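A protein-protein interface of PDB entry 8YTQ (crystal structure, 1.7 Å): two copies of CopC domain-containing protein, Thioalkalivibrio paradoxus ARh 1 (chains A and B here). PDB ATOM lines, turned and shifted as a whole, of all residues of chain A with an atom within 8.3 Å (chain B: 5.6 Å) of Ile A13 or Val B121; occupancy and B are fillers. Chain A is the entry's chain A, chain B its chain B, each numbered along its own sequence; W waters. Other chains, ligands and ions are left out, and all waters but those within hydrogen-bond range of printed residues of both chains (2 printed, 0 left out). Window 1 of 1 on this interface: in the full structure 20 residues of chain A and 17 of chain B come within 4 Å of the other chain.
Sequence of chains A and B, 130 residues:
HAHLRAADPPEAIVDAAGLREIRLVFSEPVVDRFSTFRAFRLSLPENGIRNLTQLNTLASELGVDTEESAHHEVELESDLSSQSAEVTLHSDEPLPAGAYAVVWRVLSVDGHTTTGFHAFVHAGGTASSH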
ATOM      1  N   PRO A   9      36.322  -2.271 -13.082  1.00  0.00           N
ATOM      2  CA  PRO A   9      35.787  -3.631 -13.227  1.00  0.00           C
ATOM      3  C   PRO A   9      36.552  -4.425 -14.293  1.00  0.00           C
ATOM      4  O   PRO A   9      37.078  -3.876 -15.275  1.00  0.00           O
ATOM      5  CB  PRO A   9      34.369  -3.454 -13.830  1.00  0.00           C
ATOM      6  CG  PRO A   9      34.036  -1.982 -13.568  1.00  0.00           C
ATOM      7  CD  PRO A   9      35.341  -1.239 -13.442  1.00  0.00           C
ATOM      8  N   PRO A  10      36.607  -5.752 -14.121  1.00  0.00           N
ATOM      9  CA  PRO A  10      37.218  -6.608 -15.116  1.00  0.00           C
ATOM     10  C   PRO A  10      36.190  -6.839 -16.224  1.00  0.00           C
ATOM     11  O   PRO A  10      35.086  -6.301 -16.193  1.00  0.00           O
ATOM     12  CB  PRO A  10      37.488  -7.880 -14.301  1.00  0.00           C
ATOM     13  CG  PRO A  10      36.349  -7.944 -13.333  1.00  0.00           C
ATOM     14  CD  PRO A  10      36.130  -6.496 -12.940  1.00  0.00           C
ATOM     15  N   GLU A  11      36.585  -7.603 -17.264  1.00  0.00           N
ATOM     16  CA  GLU A  11      35.661  -7.993 -18.309  1.00  0.00           C
ATOM     17  C   GLU A  11      34.703  -9.049 -17.750  1.00  0.00           C
ATOM     18  O   GLU A  11      34.987 -10.266 -17.809  1.00  0.00           O
ATOM     19  CB  GLU A  11      36.402  -8.701 -19.449  1.00  0.00           C
ATOM     20  CG  GLU A  11      35.406  -8.913 -20.586  1.00  0.00           C
ATOM     21  CD  GLU A  11      35.766  -8.761 -22.049  1.00  0.00           C
ATOM     22  OE1 GLU A  11      35.022  -7.989 -22.717  1.00  0.00           O
ATOM     23  OE2 GLU A  11      36.774  -9.382 -22.509  1.00  0.00           O
ATOM     24  N   ALA A  12      33.600  -8.560 -17.142  1.00  0.00           N
ATOM     25  CA  ALA A  12      32.579  -9.416 -16.603  1.00  0.00           C
ATOM     26  C   ALA A  12      31.277  -8.646 -16.454  1.00  0.00           C
ATOM     27  O   ALA A  12      31.259  -7.427 -16.678  1.00  0.00           O
ATOM     28  CB  ALA A  12      33.089  -9.976 -15.254  1.00  0.00           C
ATOM     29  N   ILE A  13      30.207  -9.387 -16.067  1.00  0.00           N
ATOM     30  CA  ILE A  13      28.961  -8.810 -15.632  1.00  0.00           C
ATOM     31  C   ILE A  13      29.065  -8.642 -14.118  1.00  0.00           C
ATOM     32  O   ILE A  13      29.072  -9.613 -13.399  1.00  0.00           O
ATOM     33  CB  ILE A  13      27.811  -9.780 -16.018  1.00  0.00           C
ATOM     34  CG1 ILE A  13      27.858 -10.069 -17.517  1.00  0.00           C
ATOM     35  CG2 ILE A  13      26.492  -9.083 -15.641  1.00  0.00           C
ATOM     36  CD1 ILE A  13      27.124 -11.358 -17.902  1.00  0.00           C
ATOM     37  N   VAL A  14      29.108  -7.379 -13.692  1.00  0.00           N
ATOM     38  CA  VAL A  14      29.266  -7.017 -12.270  1.00  0.00           C
ATOM     39  C   VAL A  14      27.997  -6.338 -11.777  1.00  0.00           C
ATOM     40  O   VAL A  14      27.314  -5.690 -12.568  1.00  0.00           O
ATOM     41  CB  VAL A  14      30.534  -6.179 -12.064  1.00  0.00           C
ATOM     42  CG1 VAL A  14      31.727  -7.061 -12.403  1.00  0.00           C
ATOM     43  CG2 VAL A  14      30.507  -4.850 -12.861  1.00  0.00           C
ATOM     44  N   ASP A  15      27.749  -6.480 -10.473  1.00  0.00           N
ATOM     45  CA  ASP A  15      26.637  -5.743  -9.837  1.00  0.00           C
ATOM     46  C   ASP A  15      27.154  -4.332  -9.534  1.00  0.00           C
ATOM     47  O   ASP A  15      26.857  -3.372 -10.249  1.00  0.00           O
ATOM     48  CB  ASP A  15      26.247  -6.468  -8.539  1.00  0.00           C
ATOM     49  CG  ASP A  15      24.985  -7.331  -8.568  1.00  0.00           C
ATOM     50  OD1 ASP A  15      24.050  -7.129  -9.461  1.00  0.00           O
ATOM     51  OD2 ASP A  15      24.939  -8.311  -7.751  1.00  0.00           O
ATOM     52  N   ALA A  16      27.997  -4.205  -8.466  1.00  0.00           N
ATOM     53  CA  ALA A  16      28.766  -2.976  -8.279  1.00  0.00           C
ATOM     54  C   ALA A  16      27.857  -1.740  -8.306  1.00  0.00           C
ATOM     55  O   ALA A  16      28.145  -0.768  -9.038  1.00  0.00           O
ATOM     56  CB  ALA A  16      29.864  -2.844  -9.310  1.00  0.00           C
ATOM     57  N   LEU A  44      22.971  -1.949 -27.039  1.00  0.00           N
ATOM     58  CA  LEU A  44      22.927  -3.366 -27.394  1.00  0.00           C
ATOM     59  C   LEU A  44      21.878  -3.492 -28.511  1.00  0.00           C
ATOM     60  O   LEU A  44      20.878  -2.747 -28.512  1.00  0.00           O
ATOM     61  CB  LEU A  44      22.515  -4.225 -26.186  1.00  0.00           C
ATOM     62  CG  LEU A  44      23.512  -4.231 -25.025  1.00  0.00           C
ATOM     63  CD1 LEU A  44      23.089  -5.207 -23.911  1.00  0.00           C
ATOM     64  CD2 LEU A  44      24.913  -4.613 -25.476  1.00  0.00           C
ATOM     65  N   GLY A  48      19.560  -8.457 -27.828  1.00  0.00           N
ATOM     66  CA  GLY A  48      20.565  -8.550 -26.794  1.00  0.00           C
ATOM     67  C   GLY A  48      21.833  -9.260 -27.296  1.00  0.00           C
ATOM     68  O   GLY A  48      21.932  -9.648 -28.494  1.00  0.00           O
ATOM     69  N   ILE A  49      22.808  -9.423 -26.400  1.00  0.00           N
ATOM     70  CA  ILE A  49      23.999 -10.206 -26.764  1.00  0.00           C
ATOM     71  C   ILE A  49      24.103 -11.389 -25.841  1.00  0.00           C
ATOM     72  O   ILE A  49      23.560 -11.342 -24.756  1.00  0.00           O
ATOM     73  CB  ILE A  49      25.294  -9.386 -26.729  1.00  0.00           C
ATOM     74  CG1 ILE A  49      25.499  -8.752 -25.350  1.00  0.00           C
ATOM     75  CG2 ILE A  49      25.285  -8.339 -27.863  1.00  0.00           C
ATOM     76  CD1 ILE A  49      26.904  -8.051 -25.238  1.00  0.00           C
ATOM     77  N   ARG A  50      24.722 -12.476 -26.319  1.00  0.00           N
ATOM     78  CA  ARG A  50      24.714 -13.722 -25.570  1.00  0.00           C
ATOM     79  C   ARG A  50      26.060 -13.952 -24.861  1.00  0.00           C
ATOM     80  O   ARG A  50      26.162 -14.766 -23.905  1.00  0.00           O
ATOM     81  CB  ARG A  50      24.421 -14.912 -26.476  1.00  0.00           C
ATOM     82  CG  ARG A  50      23.049 -14.802 -27.123  1.00  0.00           C
ATOM     83  N   ASN A  51      27.119 -13.216 -25.272  1.00  0.00           N
ATOM     84  CA  ASN A  51      28.380 -13.490 -24.624  1.00  0.00           C
ATOM     85  C   ASN A  51      29.265 -12.253 -24.711  1.00  0.00           C
ATOM     86  O   ASN A  51      28.953 -11.250 -25.391  1.00  0.00           O
ATOM     87  CB  ASN A  51      29.132 -14.708 -25.268  1.00  0.00           C
ATOM     88  CG  ASN A  51      29.300 -14.550 -26.767  1.00  0.00           C
ATOM     89  OD1 ASN A  51      29.953 -13.585 -27.199  1.00  0.00           O
ATOM     90  ND2 ASN A  51      28.839 -15.518 -27.574  1.00  0.00           N
ATOM     91  N   LEU A  52      30.338 -12.297 -23.923  1.00  0.00           N
ATOM     92  CA  LEU A  52      31.223 -11.120 -23.844  1.00  0.00           C
ATOM     93  C   LEU A  52      32.131 -10.933 -25.072  1.00  0.00           C
ATOM     94  O   LEU A  52      32.656  -9.823 -25.268  1.00  0.00           O
ATOM     95  CB  LEU A  52      32.003 -11.184 -22.526  1.00  0.00           C
ATOM     96  CG  LEU A  52      31.120 -11.104 -21.256  1.00  0.00           C
ATOM     97  CD1 LEU A  52      32.013 -10.763 -19.998  1.00  0.00           C
ATOM     98  CD2 LEU A  52      30.090 -10.003 -21.398  1.00  0.00           C
ATOM     99  N   LEU A  55      30.304  -8.501 -26.914  1.00  0.00           N
ATOM    100  CA  LEU A  55      30.505  -7.195 -26.302  1.00  0.00           C
ATOM    101  C   LEU A  55      31.804  -6.628 -26.859  1.00  0.00           C
ATOM    102  O   LEU A  55      31.827  -5.454 -27.231  1.00  0.00           O
ATOM    103  CB  LEU A  55      30.570  -7.337 -24.773  1.00  0.00           C
ATOM    104  CG  LEU A  55      30.835  -6.019 -24.034  1.00  0.00           C
ATOM    105  CD1 LEU A  55      29.613  -5.118 -24.132  1.00  0.00           C
ATOM    106  CD2 LEU A  55      31.132  -6.310 -22.546  1.00  0.00           C
ATOM    107  N   GLY A  98      24.475  -0.752 -17.507  1.00  0.00           N
ATOM    108  CA  GLY A  98      24.589  -0.881 -18.964  1.00  0.00           C
ATOM    109  C   GLY A  98      25.888  -1.557 -19.316  1.00  0.00           C
ATOM    110  O   GLY A  98      26.765  -1.801 -18.457  1.00  0.00           O
ATOM    111  N   ALA A 119      36.057  -3.841 -21.914  1.00  0.00           N
ATOM    112  CA  ALA A 119      34.613  -3.693 -21.820  1.00  0.00           C
ATOM    113  C   ALA A 119      34.079  -4.475 -20.607  1.00  0.00           C
ATOM    114  O   ALA A 119      34.734  -5.429 -20.176  1.00  0.00           O
ATOM    115  CB  ALA A 119      33.967  -4.223 -23.113  1.00  0.00           C
ATOM    116  N   PHE A 120      32.956  -4.020 -20.077  1.00  0.00           N
ATOM    117  CA  PHE A 120      32.293  -4.776 -18.990  1.00  0.00           C
ATOM    118  C   PHE A 120      30.784  -4.493 -19.012  1.00  0.00           C
ATOM    119  O   PHE A 120      30.344  -3.588 -19.727  1.00  0.00           O
ATOM    120  CB  PHE A 120      32.858  -4.391 -17.604  1.00  0.00           C
ATOM    121  CG  PHE A 120      32.725  -2.936 -17.255  1.00  0.00           C
ATOM    122  CD1 PHE A 120      33.772  -2.056 -17.647  1.00  0.00           C
ATOM    123  CD2 PHE A 120      31.592  -2.389 -16.668  1.00  0.00           C
ATOM    124  CE1 PHE A 120      33.636  -0.690 -17.527  1.00  0.00           C
ATOM    125  CE2 PHE A 120      31.502  -1.003 -16.413  1.00  0.00           C
ATOM    126  CZ  PHE A 120      32.570  -0.166 -16.801  1.00  0.00           C
ATOM    127  N   VAL A 121      30.008  -5.280 -18.239  1.00  0.00           N
ATOM    128  CA  VAL A 121      28.590  -5.025 -18.089  1.00  0.00           C
ATOM    129  C   VAL A 121      28.257  -4.651 -16.660  1.00  0.00           C
ATOM    130  O   VAL A 121      28.547  -5.423 -15.763  1.00  0.00           O
ATOM    131  CB  VAL A 121      27.689  -6.191 -18.545  1.00  0.00           C
ATOM    132  CG1 VAL A 121      26.220  -5.771 -18.375  1.00  0.00           C
ATOM    133  CG2 VAL A 121      27.999  -6.611 -20.029  1.00  0.00           C
ATOM    134  N   HIS A 122      27.741  -3.433 -16.464  1.00  0.00           N
ATOM    135  CA  HIS A 122      27.298  -2.969 -15.155  1.00  0.00           C
ATOM    136  C   HIS A 122      25.809  -3.375 -15.012  1.00  0.00           C
ATOM    137  O   HIS A 122      24.904  -2.692 -15.505  1.00  0.00           O
ATOM    138  CB  HIS A 122      27.541  -1.423 -15.053  1.00  0.00           C
ATOM    139  CG  HIS A 122      27.162  -0.895 -13.725  1.00  0.00           C
ATOM    140  ND1 HIS A 122      26.569   0.335 -13.513  1.00  0.00           N
ATOM    141  CD2 HIS A 122      27.243  -1.508 -12.517  1.00  0.00           C
ATOM    142  CE1 HIS A 122      26.429   0.508 -12.205  1.00  0.00           C
ATOM    143  NE2 HIS A 122      26.835  -0.614 -11.567  1.00  0.00           N
ATOM    144  N   ALA A 123      25.555  -4.489 -14.307  1.00  0.00           N
ATOM    145  CA  ALA A 123      24.173  -4.928 -14.106  1.00  0.00           C
ATOM    146  C   ALA A 123      23.560  -4.403 -12.803  1.00  0.00           C
ATOM    147  O   ALA A 123      22.497  -4.881 -12.428  1.00  0.00           O
ATOM    148  CB  ALA A 123      24.143  -6.431 -14.098  1.00  0.00           C
ATOM    149  N   GLY A 124      24.243  -3.562 -12.074  1.00  0.00           N
ATOM    150  CA  GLY A 124      23.604  -2.929 -10.930  1.00  0.00           C
ATOM    151  C   GLY A 124      23.302  -1.473 -11.268  1.00  0.00           C
ATOM    152  O   GLY A 124      23.697  -0.965 -12.330  1.00  0.00           O
ATOM    153  N   ALA B  12      19.859 -13.764 -22.623  1.00  0.00           N
ATOM    154  CA  ALA B  12      20.749 -12.781 -23.232  1.00  0.00           C
ATOM    155  C   ALA B  12      20.937 -11.634 -22.255  1.00  0.00           C
ATOM    156  O   ALA B  12      20.180 -11.542 -21.259  1.00  0.00           O
ATOM    157  CB  ALA B  12      20.114 -12.232 -24.510  1.00  0.00           C
ATOM    158  N   ILE B  13      22.021 -10.861 -22.494  1.00  0.00           N
ATOM    159  CA  ILE B  13      22.140  -9.549 -21.890  1.00  0.00           C
ATOM    160  C   ILE B  13      21.336  -8.590 -22.753  1.00  0.00           C
ATOM    161  O   ILE B  13      21.713  -8.337 -23.922  1.00  0.00           O
ATOM    162  CB  ILE B  13      23.618  -9.165 -21.817  1.00  0.00           C
ATOM    163  CG1 ILE B  13      24.492 -10.291 -21.255  1.00  0.00           C
ATOM    164  CG2 ILE B  13      23.802  -7.823 -21.085  1.00  0.00           C
ATOM    165  CD1 ILE B  13      25.946 -10.288 -21.711  1.00  0.00           C
ATOM    166  N   VAL B  14      20.261  -8.025 -22.166  1.00  0.00           N
ATOM    167  CA  VAL B  14      19.363  -7.122 -22.875  1.00  0.00           C
ATOM    168  C   VAL B  14      19.402  -5.733 -22.231  1.00  0.00           C
ATOM    169  O   VAL B  14      19.721  -5.625 -21.045  1.00  0.00           O
ATOM    170  CB  VAL B  14      17.913  -7.662 -22.938  1.00  0.00           C
ATOM    171  CG1 VAL B  14      17.911  -8.985 -23.689  1.00  0.00           C
ATOM    172  CG2 VAL B  14      17.317  -7.913 -21.554  1.00  0.00           C
ATOM    173  N   ASP B  15      19.143  -4.708 -23.055  1.00  0.00           N
ATOM    174  CA  ASP B  15      18.977  -3.362 -22.462  1.00  0.00           C
ATOM    175  C   ASP B  15      17.565  -3.251 -21.899  1.00  0.00           C
ATOM    176  O   ASP B  15      17.387  -3.355 -20.668  1.00  0.00           O
ATOM    177  CB  ASP B  15      19.420  -2.269 -23.466  1.00  0.00           C
ATOM    178  CG  ASP B  15      20.831  -1.734 -23.265  1.00  0.00           C
ATOM    179  OD1 ASP B  15      21.581  -2.216 -22.342  1.00  0.00           O
ATOM    180  OD2 ASP B  15      21.169  -0.752 -23.923  1.00  0.00           O
ATOM    181  N   LEU B  44      25.190 -11.727  -7.772  1.00  0.00           N
ATOM    182  CA  LEU B  44      26.390 -12.038  -8.497  1.00  0.00           C
ATOM    183  C   LEU B  44      27.540 -12.108  -7.486  1.00  0.00           C
ATOM    184  O   LEU B  44      27.561 -11.194  -6.646  1.00  0.00           O
ATOM    185  CB  LEU B  44      26.646 -10.835  -9.418  1.00  0.00           C
ATOM    186  CG  LEU B  44      25.642 -10.643 -10.564  1.00  0.00           C
ATOM    187  CD1 LEU B  44      26.078  -9.421 -11.426  1.00  0.00           C
ATOM    188  CD2 LEU B  44      25.658 -11.928 -11.436  1.00  0.00           C
ATOM    189  N   ASN B  47      33.140  -9.517  -8.083  1.00  0.00           N
ATOM    190  CA  ASN B  47      33.772  -9.453  -9.429  1.00  0.00           C
ATOM    191  C   ASN B  47      33.062 -10.184 -10.577  1.00  0.00           C
ATOM    192  O   ASN B  47      33.626 -10.313 -11.691  1.00  0.00           O
ATOM    193  CB  ASN B  47      35.261  -9.824  -9.473  1.00  0.00           C
ATOM    194  CG  ASN B  47      36.078  -8.703  -8.877  1.00  0.00           C
ATOM    195  OD1 ASN B  47      36.264  -7.656  -9.500  1.00  0.00           O
ATOM    196  ND2 ASN B  47      36.508  -8.915  -7.647  1.00  0.00           N
ATOM    197  N   GLY B  48      31.863 -10.673 -10.345  1.00  0.00           N
ATOM    198  CA  GLY B  48      30.908 -10.828 -11.419  1.00  0.00           C
ATOM    199  C   GLY B  48      31.032 -12.196 -12.080  1.00  0.00           C
ATOM    200  O   GLY B  48      31.781 -13.111 -11.662  1.00  0.00           O
ATOM    201  N   ILE B  49      30.221 -12.347 -13.115  1.00  0.00           N
ATOM    202  CA  ILE B  49      30.195 -13.583 -13.893  1.00  0.00           C
ATOM    203  C   ILE B  49      30.633 -13.250 -15.297  1.00  0.00           C
ATOM    204  O   ILE B  49      30.506 -12.092 -15.714  1.00  0.00           O
ATOM    205  CB  ILE B  49      28.830 -14.258 -13.912  1.00  0.00           C
ATOM    206  CG1 ILE B  49      27.732 -13.329 -14.456  1.00  0.00           C
ATOM    207  CG2 ILE B  49      28.448 -14.751 -12.513  1.00  0.00           C
ATOM    208  CD1 ILE B  49      26.335 -14.066 -14.755  1.00  0.00           C
ATOM    209  N   ARG B  50      31.186 -14.274 -16.002  1.00  0.00           N
ATOM    210  CA  ARG B  50      31.886 -13.925 -17.219  1.00  0.00           C
ATOM    211  C   ARG B  50      31.225 -14.525 -18.467  1.00  0.00           C
ATOM    212  O   ARG B  50      31.606 -14.191 -19.593  1.00  0.00           O
ATOM    213  CB  ARG B  50      33.344 -14.368 -17.070  1.00  0.00           C
ATOM    214  CG  ARG B  50      34.120 -13.697 -15.958  1.00  0.00           C
ATOM    215  CD  ARG B  50      35.628 -13.717 -16.241  1.00  0.00           C
ATOM    216  NE  ARG B  50      36.334 -12.802 -15.342  1.00  0.00           N
ATOM    217  CZ  ARG B  50      37.245 -11.880 -15.686  1.00  0.00           C
ATOM    218  NH1 ARG B  50      37.634 -11.740 -16.947  1.00  0.00           N
ATOM    219  NH2 ARG B  50      37.793 -11.115 -14.742  1.00  0.00           N
ATOM    220  N   ASN B  51      30.141 -15.283 -18.289  1.00  0.00           N
ATOM    221  CA  ASN B  51      29.303 -15.749 -19.382  1.00  0.00           C
ATOM    222  C   ASN B  51      27.987 -16.213 -18.800  1.00  0.00           C
ATOM    223  O   ASN B  51      27.745 -16.214 -17.558  1.00  0.00           O
ATOM    224  CB  ASN B  51      29.962 -16.930 -20.137  1.00  0.00           C
ATOM    225  CG  ASN B  51      30.409 -18.091 -19.257  1.00  0.00           C
ATOM    226  OD1 ASN B  51      29.625 -18.570 -18.453  1.00  0.00           O
ATOM    227  ND2 ASN B  51      31.644 -18.568 -19.430  1.00  0.00           N
ATOM    228  N   LEU B  52      27.061 -16.473 -19.745  1.00  0.00           N
ATOM    229  CA  LEU B  52      25.704 -16.832 -19.291  1.00  0.00           C
ATOM    230  C   LEU B  52      25.614 -18.271 -18.865  1.00  0.00           C
ATOM    231  O   LEU B  52      24.627 -18.626 -18.239  1.00  0.00           O
ATOM    232  CB  LEU B  52      24.635 -16.485 -20.327  1.00  0.00           C
ATOM    233  CG  LEU B  52      24.614 -15.015 -20.772  1.00  0.00           C
ATOM    234  CD1 LEU B  52      23.478 -14.715 -21.727  1.00  0.00           C
ATOM    235  CD2 LEU B  52      24.736 -14.012 -19.592  1.00  0.00           C
ATOM    236  N   LEU B  55      25.732 -17.967 -15.341  1.00  0.00           N
ATOM    237  CA  LEU B  55      24.435 -17.449 -14.877  1.00  0.00           C
ATOM    238  C   LEU B  55      23.489 -18.637 -14.794  1.00  0.00           C
ATOM    239  O   LEU B  55      22.778 -18.725 -13.764  1.00  0.00           O
ATOM    240  CB  LEU B  55      23.867 -16.422 -15.875  1.00  0.00           C
ATOM    241  CG  LEU B  55      22.424 -15.952 -15.703  1.00  0.00           C
ATOM    242  CD1 LEU B  55      22.360 -14.954 -14.578  1.00  0.00           C
ATOM    243  CD2 LEU B  55      21.936 -15.285 -17.014  1.00  0.00           C
ATOM    244  N   GLY B  98      20.093  -6.027 -13.402  1.00  0.00           N
ATOM    245  CA  GLY B  98      20.514  -7.155 -12.614  1.00  0.00           C
ATOM    246  C   GLY B  98      20.420  -8.461 -13.390  1.00  0.00           C
ATOM    247  O   GLY B  98      19.826  -8.508 -14.461  1.00  0.00           O
ATOM    248  N   ALA B  99      20.930  -9.512 -12.758  1.00  0.00           N
ATOM    249  CA  ALA B  99      20.765 -10.835 -13.328  1.00  0.00           C
ATOM    250  C   ALA B  99      19.487 -11.439 -12.756  1.00  0.00           C
ATOM    251  O   ALA B  99      19.251 -11.303 -11.544  1.00  0.00           O
ATOM    252  CB  ALA B  99      22.031 -11.596 -13.019  1.00  0.00           C
ATOM    253  N   TYR B 100      18.646 -12.077 -13.594  1.00  0.00           N
ATOM    254  CA  TYR B 100      17.368 -12.612 -13.120  1.00  0.00           C
ATOM    255  C   TYR B 100      17.155 -14.047 -13.569  1.00  0.00           C
ATOM    256  O   TYR B 100      17.645 -14.451 -14.637  1.00  0.00           O
ATOM    257  CB  TYR B 100      16.201 -11.827 -13.744  1.00  0.00           C
ATOM    258  CG  TYR B 100      16.062 -10.444 -13.142  1.00  0.00           C
ATOM    259  CD1 TYR B 100      15.305 -10.231 -11.992  1.00  0.00           C
ATOM    260  CD2 TYR B 100      16.789  -9.392 -13.665  1.00  0.00           C
ATOM    261  CE1 TYR B 100      15.210  -8.963 -11.456  1.00  0.00           C
ATOM    262  CE2 TYR B 100      16.711  -8.115 -13.123  1.00  0.00           C
ATOM    263  CZ  TYR B 100      15.891  -7.895 -12.035  1.00  0.00           C
ATOM    264  OH  TYR B 100      15.870  -6.630 -11.494  1.00  0.00           O
ATOM    265  N   ALA B 119      16.942 -17.721 -17.698  1.00  0.00           N
ATOM    266  CA  ALA B 119      17.690 -16.661 -17.009  1.00  0.00           C
ATOM    267  C   ALA B 119      18.168 -15.649 -18.020  1.00  0.00           C
ATOM    268  O   ALA B 119      18.382 -16.025 -19.205  1.00  0.00           O
ATOM    269  CB  ALA B 119      18.883 -17.180 -16.223  1.00  0.00           C
ATOM    270  N   PHE B 120      18.274 -14.395 -17.544  1.00  0.00           N
ATOM    271  CA  PHE B 120      18.752 -13.311 -18.448  1.00  0.00           C
ATOM    272  C   PHE B 120      19.443 -12.243 -17.624  1.00  0.00           C
ATOM    273  O   PHE B 120      19.351 -12.254 -16.375  1.00  0.00           O
ATOM    274  CB  PHE B 120      17.582 -12.787 -19.301  1.00  0.00           C
ATOM    275  CG  PHE B 120      16.484 -12.107 -18.526  1.00  0.00           C
ATOM    276  CD1 PHE B 120      16.534 -10.749 -18.268  1.00  0.00           C
ATOM    277  CD2 PHE B 120      15.454 -12.878 -17.964  1.00  0.00           C
ATOM    278  CE1 PHE B 120      15.551 -10.164 -17.462  1.00  0.00           C
ATOM    279  CE2 PHE B 120      14.460 -12.299 -17.161  1.00  0.00           C
ATOM    280  CZ  PHE B 120      14.551 -10.959 -16.892  1.00  0.00           C
ATOM    281  N   VAL B 121      20.117 -11.321 -18.339  1.00  0.00           N
ATOM    282  CA  VAL B 121      20.782 -10.207 -17.660  1.00  0.00           C
ATOM    283  C   VAL B 121      20.096  -8.947 -18.145  1.00  0.00           C
ATOM    284  O   VAL B 121      20.054  -8.656 -19.340  1.00  0.00           O
ATOM    285  CB  VAL B 121      22.312 -10.147 -17.867  1.00  0.00           C
ATOM    286  CG1 VAL B 121      22.817  -8.909 -17.135  1.00  0.00           C
ATOM    287  CG2 VAL B 121      22.917 -11.393 -17.286  1.00  0.00           C
ATOM    288  N   HIS B 122      19.543  -8.187 -17.175  1.00  0.00           N
ATOM    289  CA  HIS B 122      18.954  -6.905 -17.552  1.00  0.00           C
ATOM    290  C   HIS B 122      20.030  -5.829 -17.369  1.00  0.00           C
ATOM    291  O   HIS B 122      20.359  -5.435 -16.225  1.00  0.00           O
ATOM    292  CB  HIS B 122      17.762  -6.592 -16.573  1.00  0.00           C
ATOM    293  CG  HIS B 122      16.975  -5.416 -17.011  1.00  0.00           C
ATOM    294  ND1 HIS B 122      16.261  -4.637 -16.121  1.00  0.00           N
ATOM    295  CD2 HIS B 122      16.781  -4.871 -18.231  1.00  0.00           C
ATOM    296  CE1 HIS B 122      15.662  -3.689 -16.762  1.00  0.00           C
ATOM    297  NE2 HIS B 122      15.920  -3.811 -18.045  1.00  0.00           N
ATOM    298  N   ALA B 123      20.625  -5.353 -18.506  1.00  0.00           N
ATOM    299  CA  ALA B 123      21.648  -4.292 -18.424  1.00  0.00           C
ATOM    300  C   ALA B 123      21.081  -2.875 -18.478  1.00  0.00           C
ATOM    301  O   ALA B 123      21.815  -1.890 -18.272  1.00  0.00           O
ATOM    302  CB  ALA B 123      22.674  -4.493 -19.477  1.00  0.00           C
HETATM  303  O   HOH W   1      21.701  -9.132  -9.918  1.00  0.00           O
HETATM  304  O   HOH W   2      27.760 -16.337 -22.323  1.00  0.00           O
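Among the printed residues, merely in contact across the chains: Pro A10 with Asn B47 (3.6 Å), Pro A10 with Arg B50 (3.3 Å), Ala A12 with Asn B47 (3.6 Å), Ala A12 with Ile B49 (3.4 Å), Ala A12 with Arg B50 (3.9 Å), Ile A13 with Leu B44 (3.6 Å), Ile A13 with Gly B48 (3.0 Å), Ile A13 with Leu B52 (3.9 Å), Ile A13 with Val B121 (3.97 Å), Val A14 with Leu B44 (3.6 Å), Val A14 with Asn B47 (3.8 Å), Val A14 with Gly B48 (3.98 Å), Leu A44 with Ile B13 (3.4 Å), Leu A44 with Asp B15 (3.7 Å), Gly A48 with Ile B13 (3.1 Å), Ile A49 with Ala B12 (3.5 Å), Arg A50 with Leu B52 (3.5 Å), Leu A52 with Arg B50 (3.5 Å) and Val A121 with Ala B123 (3.9 Å).
OD2 of Asp A15 is in hydrogen-bond range of N of Leu B44 (3.4 Å). The backbone carbonyl oxygen of Ala A123 sits at hydrogen-bond distance from the backbone NH of Gly B98, at 2.8 Å. The backbone carbonyl oxygen of Ala B123 is in hydrogen-bond range of the backbone NH of Gly A98, 3.0 Å away. The backbone NH of Ile A13 is in hydrogen-bond range of the backbone carbonyl oxygen of Ile B49. The backbone carbonyl oxygen (O) of Glu A11 sits at hydrogen-bond distance from the guanidinium group (NH1) of Arg B50. The backbone NH (N) of Ile B13 lies within hydrogen-bond range of the backbone carbonyl oxygen (O) of Ile A49, 2.8 Å away.
O of Ala B12 sits at hydrogen-bond distance from N of Val B121 (2.9 Å). The backbone NH of Val A14 lies within hydrogen-bond range of the backbone carbonyl oxygen of Val A121 (2.9 Å). The backbone NH of Val B14 lies within hydrogen-bond range of the backbone carbonyl oxygen of Val B121.
Ala A12 touches Ile B49, and with the chains exchanged Ile A49 touches Ala B12. Ile A13 touches Ile B49, and with the chains exchanged Ile A49 touches Ile B13. Val A14 touches Leu B44, but with the chains exchanged Leu A44 does not touch Val B14 (4.1 Å). Arg A50 touches Leu B52, and with the chains exchanged Leu A52 touches Arg B50.
Of the printed residues of chain B, Glu A11 touches Arg B50 (3.1 Å). Ile A13 touches five residues of chain B. Of the printed residues of chain B, Val A14 touches Leu B44, Asn B47 and Gly B48. Asn A51 touches none of the printed residues of chain B. Of the printed residues of chain A, Ile B49 touches Ala A12 and Ile A13. Of chain A, only Ile A13 (3.97 Å) comes within 4 Å of Val B121. The nearest residue of chain A that does not touch Val B121 is Ala A123 (4.1 Å).
Water W2 bridges the backbone NH of Leu B52 (2.7 Å) and the backbone carbonyl oxygen of Arg A50 (2.7 Å). Water W1 bridges the backbone NH (N) of Ala B99 (3.0 Å) and the side-chain carboxylate (OD1) of Asp A15 (3.1 Å).
Hydrophobic or aromatic side chains of chain A within 4 Å of the printed part of chain B: Pro A10, Ala A12, Ile A13, Val A14, Leu A44, Ile A49, Leu A52, Val A121 and Ala A123. Printed residues of chain B that touch a printed residue of chain A: Ala B12, Ile B13, Asp B15, Leu B44, Asn B47, Gly B48, Ile B49, Arg B50, Leu B52, Gly B98, Val B121 and Ala B123. Hydrophobic or aromatic side chains of chain B within 4 Å of the printed part of chain A: Ala B12, Ile B13, Leu B44, Ile B49, Leu B52, Val B121 and Ala B123.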
